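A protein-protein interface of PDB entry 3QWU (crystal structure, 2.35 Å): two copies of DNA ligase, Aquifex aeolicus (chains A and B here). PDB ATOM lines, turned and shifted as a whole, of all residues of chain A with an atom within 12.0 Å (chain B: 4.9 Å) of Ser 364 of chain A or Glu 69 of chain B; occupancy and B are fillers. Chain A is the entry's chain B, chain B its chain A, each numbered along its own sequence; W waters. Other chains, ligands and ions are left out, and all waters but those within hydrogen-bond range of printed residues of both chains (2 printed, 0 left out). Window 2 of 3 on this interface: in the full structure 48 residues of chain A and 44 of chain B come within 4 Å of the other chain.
Leu 62 of chain B touches Leu 362 of chain A. Leu 363 of chain A touches Leu 62 of chain B. CG2 of Thr 65 of chain B touches O of Leu 363 of chain A, at 3.7 Å. Ser 364 of chain A touches Thr 65 of chain B. Gly 365 of chain A touches Thr 65 of chain B. Gly 66 of chain B touches Gly 365 of chain A (CA to O, 3.6 Å). CB of Glu 69 of chain B touches O of Gly 365 of chain A (3.7 Å). Gly 366 of chain A touches Gln 70 of chain B. Ile 367 of chain A touches Gln 70 of chain B.
The backbone carbonyl oxygen (O) of Gly 365 of chain A lies close to the side-chain amide oxygen (OE1) of Gln 70 of chain B. The side-chain carboxylate (OE1) of Glu 69 of chain B sits close to the backbone carbonyl oxygen (O) of Ser 364 of chain A (3.2 Å).
No position is printed for both chains. Of the 11 pairs that touch across the chains among the printed residues, none has its exchanged pair printed and touching as well.
Of the 8 printed residues of chain B, 5 touch a printed residue of chain A. Printed residues of chain B that touch a printed residue of chain A: Leu 62, Thr 65, Gly 66, Glu 69 and Gln 70. Hydrophobic or aromatic side chains of chain A within 4 Å of the printed part of chain B: Leu 363 and Ile 367. Among the printed residues, no Asp or Glu carboxylate lies within 4 Å of a Lys or Arg side-chain nitrogen of the other chain.
Glu 297 of chain A touches none of the printed residues of chain B. Of the printed residues of chain B, Leu 363 of chain A touches Leu 62 (3.4 Å) and Thr 65 (3.7 Å). Ser 364 of chain A touches just these residues of chain B: Thr 65 (3.3 Å) and Glu 69 (3.2 Å). Of the printed residues of chain B, Gly 365 of chain A touches Thr 65 (3.5 Å), Gly 66 (3.6 Å), Glu 69 (3.7 Å) and Gln 70 (3.2 Å). Of the printed residues of chain B, Ile 367 of chain A touches Gln 70 (3.3 Å). Of the printed residues of chain A, Leu 62 of chain B touches Leu 362 (3.8 Å) and Leu 363 (3.4 Å). Thr 65 of chain B touches just these residues of chain A: Leu 363 (3.7 Å), Ser 364 (3.3 Å) and Gly 365 (3.5 Å). Of the printed residues of chain A, Gly 66 of chain B touches Gly 365 (3.6 Å). Leu 67 of chain B touches none of the printed residues of chain A. Glu 69 of chain B touches just these residues of chain A: Ser 364 (3.2 Å) and Gly 365 (3.7 Å). Of the printed residues of chain A, Gln 70 of chain B touches Gly 365 (3.2 Å), Gly 366 (3.8 Å) and Ile 367 (3.3 Å). The nearest residue of chain A that does not touch Glu 69 of chain B is Gly 366 of chain A (4.8 Å).
O of Gly 360 of chain A sits at hydrogen-bond distance from OG of Ser 364 of chain A, 3.3 Å away. O of His 361 of chain A sits at hydrogen-bond distance from OG of Ser 364 of chain A. The backbone NH (N) of Gly 366 of chain A lies within hydrogen-bond range of the backbone carbonyl oxygen (O) of His 361 of chain A. A ring nitrogen (NE2) of His 361 of chain A is in hydrogen-bond range of the backbone carbonyl oxygen of Ile 367 of chain A (2.8 Å).
Water W2 lies within hydrogen-bond range of the backbone carbonyl oxygen (O) of Gly 366 of chain A, the backbone carbonyl oxygen (O) of Leu 362 of chain A and the backbone NH (N) of Leu 62 of chain B. Water W1 bridges the backbone NH (N) of Ile 367 of chain A (3.1 Å) and the side-chain amide oxygen (OE1) of Gln 70 of chain B (3.3 Å).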
ATOM      1  N   ILE A 293     -26.409  -1.837  23.063  1.00  0.00           N
ATOM      2  CA  ILE A 293     -25.389  -2.850  22.756  1.00  0.00           C
ATOM      3  C   ILE A 293     -24.038  -2.217  22.403  1.00  0.00           C
ATOM      4  O   ILE A 293     -22.995  -2.605  22.958  1.00  0.00           O
ATOM      5  CB  ILE A 293     -25.832  -3.779  21.632  1.00  0.00           C
ATOM      6  CG1 ILE A 293     -27.016  -4.636  22.076  1.00  0.00           C
ATOM      7  CG2 ILE A 293     -24.751  -4.745  21.253  1.00  0.00           C
ATOM      8  CD1 ILE A 293     -27.822  -5.161  20.928  1.00  0.00           C
ATOM      9  N   PHE A 296     -22.500  -0.952  25.577  1.00  0.00           N
ATOM     10  CA  PHE A 296     -21.947  -2.066  26.353  1.00  0.00           C
ATOM     11  C   PHE A 296     -20.636  -2.607  25.794  1.00  0.00           C
ATOM     12  O   PHE A 296     -19.754  -2.904  26.563  1.00  0.00           O
ATOM     13  CB  PHE A 296     -22.950  -3.217  26.534  1.00  0.00           C
ATOM     14  CG  PHE A 296     -22.404  -4.346  27.354  1.00  0.00           C
ATOM     15  CD1 PHE A 296     -21.676  -5.360  26.756  1.00  0.00           C
ATOM     16  CD2 PHE A 296     -22.571  -4.359  28.728  1.00  0.00           C
ATOM     17  CE1 PHE A 296     -21.178  -6.358  27.493  1.00  0.00           C
ATOM     18  CE2 PHE A 296     -22.065  -5.344  29.481  1.00  0.00           C
ATOM     19  CZ  PHE A 296     -21.363  -6.366  28.866  1.00  0.00           C
ATOM     20  N   GLU A 297     -20.491  -2.765  24.483  1.00  0.00           N
ATOM     21  CA  GLU A 297     -19.211  -3.181  23.900  1.00  0.00           C
ATOM     22  C   GLU A 297     -18.114  -2.203  24.298  1.00  0.00           C
ATOM     23  O   GLU A 297     -17.016  -2.576  24.649  1.00  0.00           O
ATOM     24  CB  GLU A 297     -19.248  -3.181  22.364  1.00  0.00           C
ATOM     25  CG  GLU A 297     -20.205  -4.131  21.669  1.00  0.00           C
ATOM     26  CD  GLU A 297     -19.649  -4.616  20.328  1.00  0.00           C
ATOM     27  OE1 GLU A 297     -20.163  -4.236  19.245  1.00  0.00           O
ATOM     28  OE2 GLU A 297     -18.672  -5.387  20.363  1.00  0.00           O
ATOM     29  N   HIS A 300     -18.662  -1.309  28.803  1.00  0.00           N
ATOM     30  CA  HIS A 300     -19.053  -2.407  29.696  1.00  0.00           C
ATOM     31  C   HIS A 300     -20.126  -2.040  30.742  1.00  0.00           C
ATOM     32  O   HIS A 300     -20.255  -2.651  31.809  1.00  0.00           O
ATOM     33  CB  HIS A 300     -17.809  -3.133  30.267  1.00  0.00           C
ATOM     34  CG  HIS A 300     -17.497  -4.417  29.538  1.00  0.00           C
ATOM     35  ND1 HIS A 300     -17.254  -5.614  30.187  1.00  0.00           N
ATOM     36  CD2 HIS A 300     -17.458  -4.695  28.209  1.00  0.00           C
ATOM     37  CE1 HIS A 300     -17.056  -6.566  29.288  1.00  0.00           C
ATOM     38  NE2 HIS A 300     -17.177  -6.034  28.080  1.00  0.00           N
ATOM     39  N   MET A 355     -30.036  -4.217  32.886  1.00  0.00           N
ATOM     40  CA  MET A 355     -29.829  -4.257  31.419  1.00  0.00           C
ATOM     41  C   MET A 355     -28.355  -4.502  31.118  1.00  0.00           C
ATOM     42  O   MET A 355     -28.023  -5.246  30.226  1.00  0.00           O
ATOM     43  CB  MET A 355     -30.279  -2.970  30.738  1.00  0.00           C
ATOM     44  CG  MET A 355     -30.063  -2.951  29.228  1.00  0.00           C
ATOM     45  SD  MET A 355     -31.108  -4.124  28.352  1.00  0.00           S
ATOM     46  CE  MET A 355     -32.666  -3.225  28.488  1.00  0.00           C
ATOM     47  N   THR A 356     -27.475  -3.885  31.883  1.00  0.00           N
ATOM     48  CA  THR A 356     -26.050  -4.144  31.768  1.00  0.00           C
ATOM     49  C   THR A 356     -25.717  -5.645  31.923  1.00  0.00           C
ATOM     50  O   THR A 356     -24.995  -6.198  31.089  1.00  0.00           O
ATOM     51  CB  THR A 356     -25.268  -3.288  32.800  1.00  0.00           C
ATOM     52  OG1 THR A 356     -25.368  -1.915  32.433  1.00  0.00           O
ATOM     53  CG2 THR A 356     -23.780  -3.706  32.899  1.00  0.00           C
ATOM     54  N   GLY A 357     -26.262  -6.296  32.956  1.00  0.00           N
ATOM     55  CA  GLY A 357     -26.078  -7.745  33.171  1.00  0.00           C
ATOM     56  C   GLY A 357     -26.785  -8.624  32.145  1.00  0.00           C
ATOM     57  O   GLY A 357     -26.254  -9.622  31.661  1.00  0.00           O
ATOM     58  N   LEU A 358     -27.971  -8.245  31.744  1.00  0.00           N
ATOM     59  CA  LEU A 358     -28.603  -9.013  30.697  1.00  0.00           C
ATOM     60  C   LEU A 358     -27.804  -8.961  29.366  1.00  0.00           C
ATOM     61  O   LEU A 358     -27.609  -9.988  28.740  1.00  0.00           O
ATOM     62  CB  LEU A 358     -30.010  -8.559  30.498  1.00  0.00           C
ATOM     63  CG  LEU A 358     -30.725  -9.390  29.449  1.00  0.00           C
ATOM     64  CD1 LEU A 358     -31.007 -10.761  30.024  1.00  0.00           C
ATOM     65  CD2 LEU A 358     -31.983  -8.703  29.068  1.00  0.00           C
ATOM     66  N   LEU A 359     -27.310  -7.795  28.947  1.00  0.00           N
ATOM     67  CA  LEU A 359     -26.682  -7.712  27.620  1.00  0.00           C
ATOM     68  C   LEU A 359     -25.340  -8.415  27.624  1.00  0.00           C
ATOM     69  O   LEU A 359     -24.968  -9.068  26.649  1.00  0.00           O
ATOM     70  CB  LEU A 359     -26.543  -6.258  27.134  1.00  0.00           C
ATOM     71  CG  LEU A 359     -27.904  -5.638  26.771  1.00  0.00           C
ATOM     72  CD1 LEU A 359     -27.824  -4.146  26.448  1.00  0.00           C
ATOM     73  CD2 LEU A 359     -28.561  -6.394  25.599  1.00  0.00           C
ATOM     74  N   GLY A 360     -24.616  -8.309  28.737  1.00  0.00           N
ATOM     75  CA  GLY A 360     -23.324  -8.987  28.863  1.00  0.00           C
ATOM     76  C   GLY A 360     -23.464 -10.479  28.953  1.00  0.00           C
ATOM     77  O   GLY A 360     -22.564 -11.221  28.557  1.00  0.00           O
ATOM     78  N   HIS A 361     -24.561 -10.929  29.537  1.00  0.00           N
ATOM     79  CA  HIS A 361     -24.841 -12.327  29.592  1.00  0.00           C
ATOM     80  C   HIS A 361     -25.219 -12.844  28.184  1.00  0.00           C
ATOM     81  O   HIS A 361     -24.680 -13.833  27.723  1.00  0.00           O
ATOM     82  CB  HIS A 361     -25.963 -12.551  30.589  1.00  0.00           C
ATOM     83  CG  HIS A 361     -26.388 -13.979  30.715  1.00  0.00           C
ATOM     84  ND1 HIS A 361     -25.629 -14.927  31.366  1.00  0.00           N
ATOM     85  CD2 HIS A 361     -27.503 -14.619  30.293  1.00  0.00           C
ATOM     86  CE1 HIS A 361     -26.252 -16.089  31.336  1.00  0.00           C
ATOM     87  NE2 HIS A 361     -27.388 -15.931  30.684  1.00  0.00           N
ATOM     88  N   LEU A 362     -26.120 -12.150  27.495  1.00  0.00           N
ATOM     89  CA  LEU A 362     -26.495 -12.525  26.139  1.00  0.00           C
ATOM     90  C   LEU A 362     -25.321 -12.448  25.151  1.00  0.00           C
ATOM     91  O   LEU A 362     -25.073 -13.426  24.430  1.00  0.00           O
ATOM     92  CB  LEU A 362     -27.680 -11.699  25.638  1.00  0.00           C
ATOM     93  CG  LEU A 362     -29.006 -11.841  26.391  1.00  0.00           C
ATOM     94  CD1 LEU A 362     -30.046 -11.057  25.658  1.00  0.00           C
ATOM     95  CD2 LEU A 362     -29.457 -13.296  26.601  1.00  0.00           C
ATOM     96  N   LEU A 363     -24.576 -11.342  25.167  1.00  0.00           N
ATOM     97  CA  LEU A 363     -23.443 -11.115  24.218  1.00  0.00           C
ATOM     98  C   LEU A 363     -22.317 -12.110  24.342  1.00  0.00           C
ATOM     99  O   LEU A 363     -21.553 -12.336  23.403  1.00  0.00           O
ATOM    100  CB  LEU A 363     -22.869  -9.690  24.301  1.00  0.00           C
ATOM    101  CG  LEU A 363     -23.870  -8.669  23.731  1.00  0.00           C
ATOM    102  CD1 LEU A 363     -23.571  -7.297  24.295  1.00  0.00           C
ATOM    103  CD2 LEU A 363     -23.989  -8.649  22.159  1.00  0.00           C
ATOM    104  N   SER A 364     -22.207 -12.721  25.503  1.00  0.00           N
ATOM    105  CA  SER A 364     -21.121 -13.639  25.737  1.00  0.00           C
ATOM    106  C   SER A 364     -21.553 -15.066  25.411  1.00  0.00           C
ATOM    107  O   SER A 364     -20.775 -15.990  25.553  1.00  0.00           O
ATOM    108  CB  SER A 364     -20.679 -13.524  27.194  1.00  0.00           C
ATOM    109  OG  SER A 364     -21.573 -14.284  28.014  1.00  0.00           O
ATOM    110  N   GLY A 365     -22.809 -15.234  25.015  1.00  0.00           N
ATOM    111  CA  GLY A 365     -23.330 -16.514  24.570  1.00  0.00           C
ATOM    112  C   GLY A 365     -24.166 -17.224  25.608  1.00  0.00           C
ATOM    113  O   GLY A 365     -24.313 -18.424  25.529  1.00  0.00           O
ATOM    114  N   GLY A 366     -24.701 -16.489  26.583  1.00  0.00           N
ATOM    115  CA  GLY A 366     -25.450 -17.071  27.678  1.00  0.00           C
ATOM    116  C   GLY A 366     -26.803 -17.605  27.244  1.00  0.00           C
ATOM    117  O   GLY A 366     -27.297 -17.304  26.158  1.00  0.00           O
ATOM    118  N   ILE A 367     -27.410 -18.374  28.133  1.00  0.00           N
ATOM    119  CA  ILE A 367     -28.723 -18.929  27.958  1.00  0.00           C
ATOM    120  C   ILE A 367     -29.745 -18.155  28.823  1.00  0.00           C
ATOM    121  O   ILE A 367     -29.429 -17.742  29.915  1.00  0.00           O
ATOM    122  CB  ILE A 367     -28.645 -20.420  28.363  1.00  0.00           C
ATOM    123  CG1 ILE A 367     -28.917 -21.332  27.175  1.00  0.00           C
ATOM    124  CG2 ILE A 367     -29.507 -20.737  29.587  1.00  0.00           C
ATOM    125  CD1 ILE A 367     -28.583 -22.850  27.511  1.00  0.00           C
ATOM    126  N   VAL A 368     -30.965 -17.975  28.339  1.00  0.00           N
ATOM    127  CA  VAL A 368     -32.042 -17.337  29.084  1.00  0.00           C
ATOM    128  C   VAL A 368     -33.289 -18.234  28.924  1.00  0.00           C
ATOM    129  O   VAL A 368     -33.470 -18.854  27.873  1.00  0.00           O
ATOM    130  CB  VAL A 368     -32.341 -15.921  28.510  1.00  0.00           C
ATOM    131  CG1 VAL A 368     -33.626 -15.397  29.064  1.00  0.00           C
ATOM    132  CG2 VAL A 368     -31.191 -14.953  28.818  1.00  0.00           C
ATOM    133  N   TYR A 369     -34.163 -18.296  29.930  1.00  0.00           N
ATOM    134  CA  TYR A 369     -35.300 -19.209  29.882  1.00  0.00           C
ATOM    135  C   TYR A 369     -36.643 -18.584  29.495  1.00  0.00           C
ATOM    136  O   TYR A 369     -36.845 -17.401  29.708  1.00  0.00           O
ATOM    137  CB  TYR A 369     -35.398 -19.947  31.199  1.00  0.00           C
ATOM    138  CG  TYR A 369     -34.267 -20.942  31.334  1.00  0.00           C
ATOM    139  CD1 TYR A 369     -34.358 -22.209  30.766  1.00  0.00           C
ATOM    140  CD2 TYR A 369     -33.094 -20.599  31.993  1.00  0.00           C
ATOM    141  CE1 TYR A 369     -33.327 -23.088  30.858  1.00  0.00           C
ATOM    142  CE2 TYR A 369     -32.051 -21.483  32.088  1.00  0.00           C
ATOM    143  CZ  TYR A 369     -32.163 -22.716  31.519  1.00  0.00           C
ATOM    144  OH  TYR A 369     -31.108 -23.601  31.645  1.00  0.00           O
ATOM    145  N   LEU B  62     -27.325 -15.398  20.494  1.00  0.00           N
ATOM    146  CA  LEU B  62     -26.215 -15.235  19.531  1.00  0.00           C
ATOM    147  C   LEU B  62     -25.897 -16.629  19.110  1.00  0.00           C
ATOM    148  O   LEU B  62     -25.673 -17.497  19.940  1.00  0.00           O
ATOM    149  CB  LEU B  62     -24.992 -14.540  20.146  1.00  0.00           C
ATOM    150  CG  LEU B  62     -25.092 -13.016  20.267  1.00  0.00           C
ATOM    151  CD1 LEU B  62     -23.883 -12.378  20.990  1.00  0.00           C
ATOM    152  CD2 LEU B  62     -25.244 -12.388  18.888  1.00  0.00           C
ATOM    153  N   THR B  65     -21.545 -17.308  19.206  1.00  0.00           N
ATOM    154  CA  THR B  65     -21.026 -17.252  20.557  1.00  0.00           C
ATOM    155  C   THR B  65     -21.836 -18.124  21.505  1.00  0.00           C
ATOM    156  O   THR B  65     -21.319 -18.551  22.485  1.00  0.00           O
ATOM    157  CB  THR B  65     -21.032 -15.813  21.049  1.00  0.00           C
ATOM    158  OG1 THR B  65     -20.397 -15.007  20.050  1.00  0.00           O
ATOM    159  CG2 THR B  65     -20.298 -15.666  22.335  1.00  0.00           C
ATOM    160  N   GLY B  66     -23.111 -18.382  21.228  1.00  0.00           N
ATOM    161  CA  GLY B  66     -23.897 -19.239  22.093  1.00  0.00           C
ATOM    162  C   GLY B  66     -23.474 -20.696  21.983  1.00  0.00           C
ATOM    163  O   GLY B  66     -23.292 -21.398  22.993  1.00  0.00           O
ATOM    164  N   LEU B  67     -23.313 -21.145  20.743  1.00  0.00           N
ATOM    165  CA  LEU B  67     -22.904 -22.510  20.476  1.00  0.00           C
ATOM    166  C   LEU B  67     -21.518 -22.782  21.050  1.00  0.00           C
ATOM    167  O   LEU B  67     -21.298 -23.770  21.714  1.00  0.00           O
ATOM    168  CB  LEU B  67     -22.903 -22.764  18.976  1.00  0.00           C
ATOM    169  CG  LEU B  67     -24.271 -22.889  18.323  1.00  0.00           C
ATOM    170  CD1 LEU B  67     -24.068 -23.384  16.898  1.00  0.00           C
ATOM    171  CD2 LEU B  67     -25.119 -23.813  19.148  1.00  0.00           C
ATOM    172  N   ARG B  68     -20.621 -21.852  20.831  1.00  0.00           N
ATOM    173  CA  ARG B  68     -19.286 -21.874  21.393  1.00  0.00           C
ATOM    174  C   ARG B  68     -19.286 -21.850  22.931  1.00  0.00           C
ATOM    175  O   ARG B  68     -18.474 -22.495  23.554  1.00  0.00           O
ATOM    176  CB  ARG B  68     -18.519 -20.700  20.804  1.00  0.00           C
ATOM    177  CG  ARG B  68     -17.054 -20.693  20.999  1.00  0.00           C
ATOM    178  CD  ARG B  68     -16.385 -19.738  19.972  1.00  0.00           C
ATOM    179  NE  ARG B  68     -16.253 -20.439  18.689  1.00  0.00           N
ATOM    180  CZ  ARG B  68     -16.310 -19.895  17.474  1.00  0.00           C
ATOM    181  NH1 ARG B  68     -16.514 -18.593  17.324  1.00  0.00           N
ATOM    182  NH2 ARG B  68     -16.154 -20.681  16.395  1.00  0.00           N
ATOM    183  N   GLU B  69     -20.216 -21.136  23.545  1.00  0.00           N
ATOM    184  CA  GLU B  69     -20.235 -21.069  25.024  1.00  0.00           C
ATOM    185  C   GLU B  69     -20.937 -22.272  25.696  1.00  0.00           C
ATOM    186  O   GLU B  69     -20.490 -22.754  26.732  1.00  0.00           O
ATOM    187  CB  GLU B  69     -20.868 -19.747  25.487  1.00  0.00           C
ATOM    188  CG  GLU B  69     -21.032 -19.545  27.011  1.00  0.00           C
ATOM    189  CD  GLU B  69     -19.755 -19.043  27.715  1.00  0.00           C
ATOM    190  OE1 GLU B  69     -19.040 -18.158  27.194  1.00  0.00           O
ATOM    191  OE2 GLU B  69     -19.483 -19.522  28.817  1.00  0.00           O
ATOM    192  N   GLN B  70     -22.036 -22.744  25.128  1.00  0.00           N
ATOM    193  CA  GLN B  70     -22.877 -23.675  25.860  1.00  0.00           C
ATOM    194  C   GLN B  70     -22.468 -25.144  25.770  1.00  0.00           C
ATOM    195  O   GLN B  70     -22.856 -25.917  26.632  1.00  0.00           O
ATOM    196  CB  GLN B  70     -24.323 -23.542  25.420  1.00  0.00           C
ATOM    197  CG  GLN B  70     -24.937 -22.211  25.786  1.00  0.00           C
ATOM    198  CD  GLN B  70     -24.901 -21.903  27.276  1.00  0.00           C
ATOM    199  OE1 GLN B  70     -24.537 -20.787  27.684  1.00  0.00           O
ATOM    200  NE2 GLN B  70     -25.305 -22.883  28.092  1.00  0.00           N
ATOM    201  N   PHE B  71     -21.689 -25.509  24.751  1.00  0.00           N
ATOM    202  CA  PHE B  71     -21.430 -26.911  24.416  1.00  0.00           C
ATOM    203  C   PHE B  71     -19.951 -27.244  24.433  1.00  0.00           C
ATOM    204  O   PHE B  71     -19.147 -26.479  23.915  1.00  0.00           O
ATOM    205  CB  PHE B  71     -22.053 -27.302  23.062  1.00  0.00           C
ATOM    206  CG  PHE B  71     -23.567 -27.195  23.046  1.00  0.00           C
ATOM    207  CD1 PHE B  71     -24.346 -28.021  23.837  1.00  0.00           C
ATOM    208  CD2 PHE B  71     -24.198 -26.265  22.267  1.00  0.00           C
ATOM    209  CE1 PHE B  71     -25.748 -27.908  23.844  1.00  0.00           C
ATOM    210  CE2 PHE B  71     -25.598 -26.126  22.299  1.00  0.00           C
ATOM    211  CZ  PHE B  71     -26.366 -26.950  23.092  1.00  0.00           C
HETATM  212  O   HOH W   1     -25.588 -19.332  30.439  1.00  0.00           O
HETATM  213  O   HOH W   2     -26.899 -15.734  23.790  1.00  0.00           O
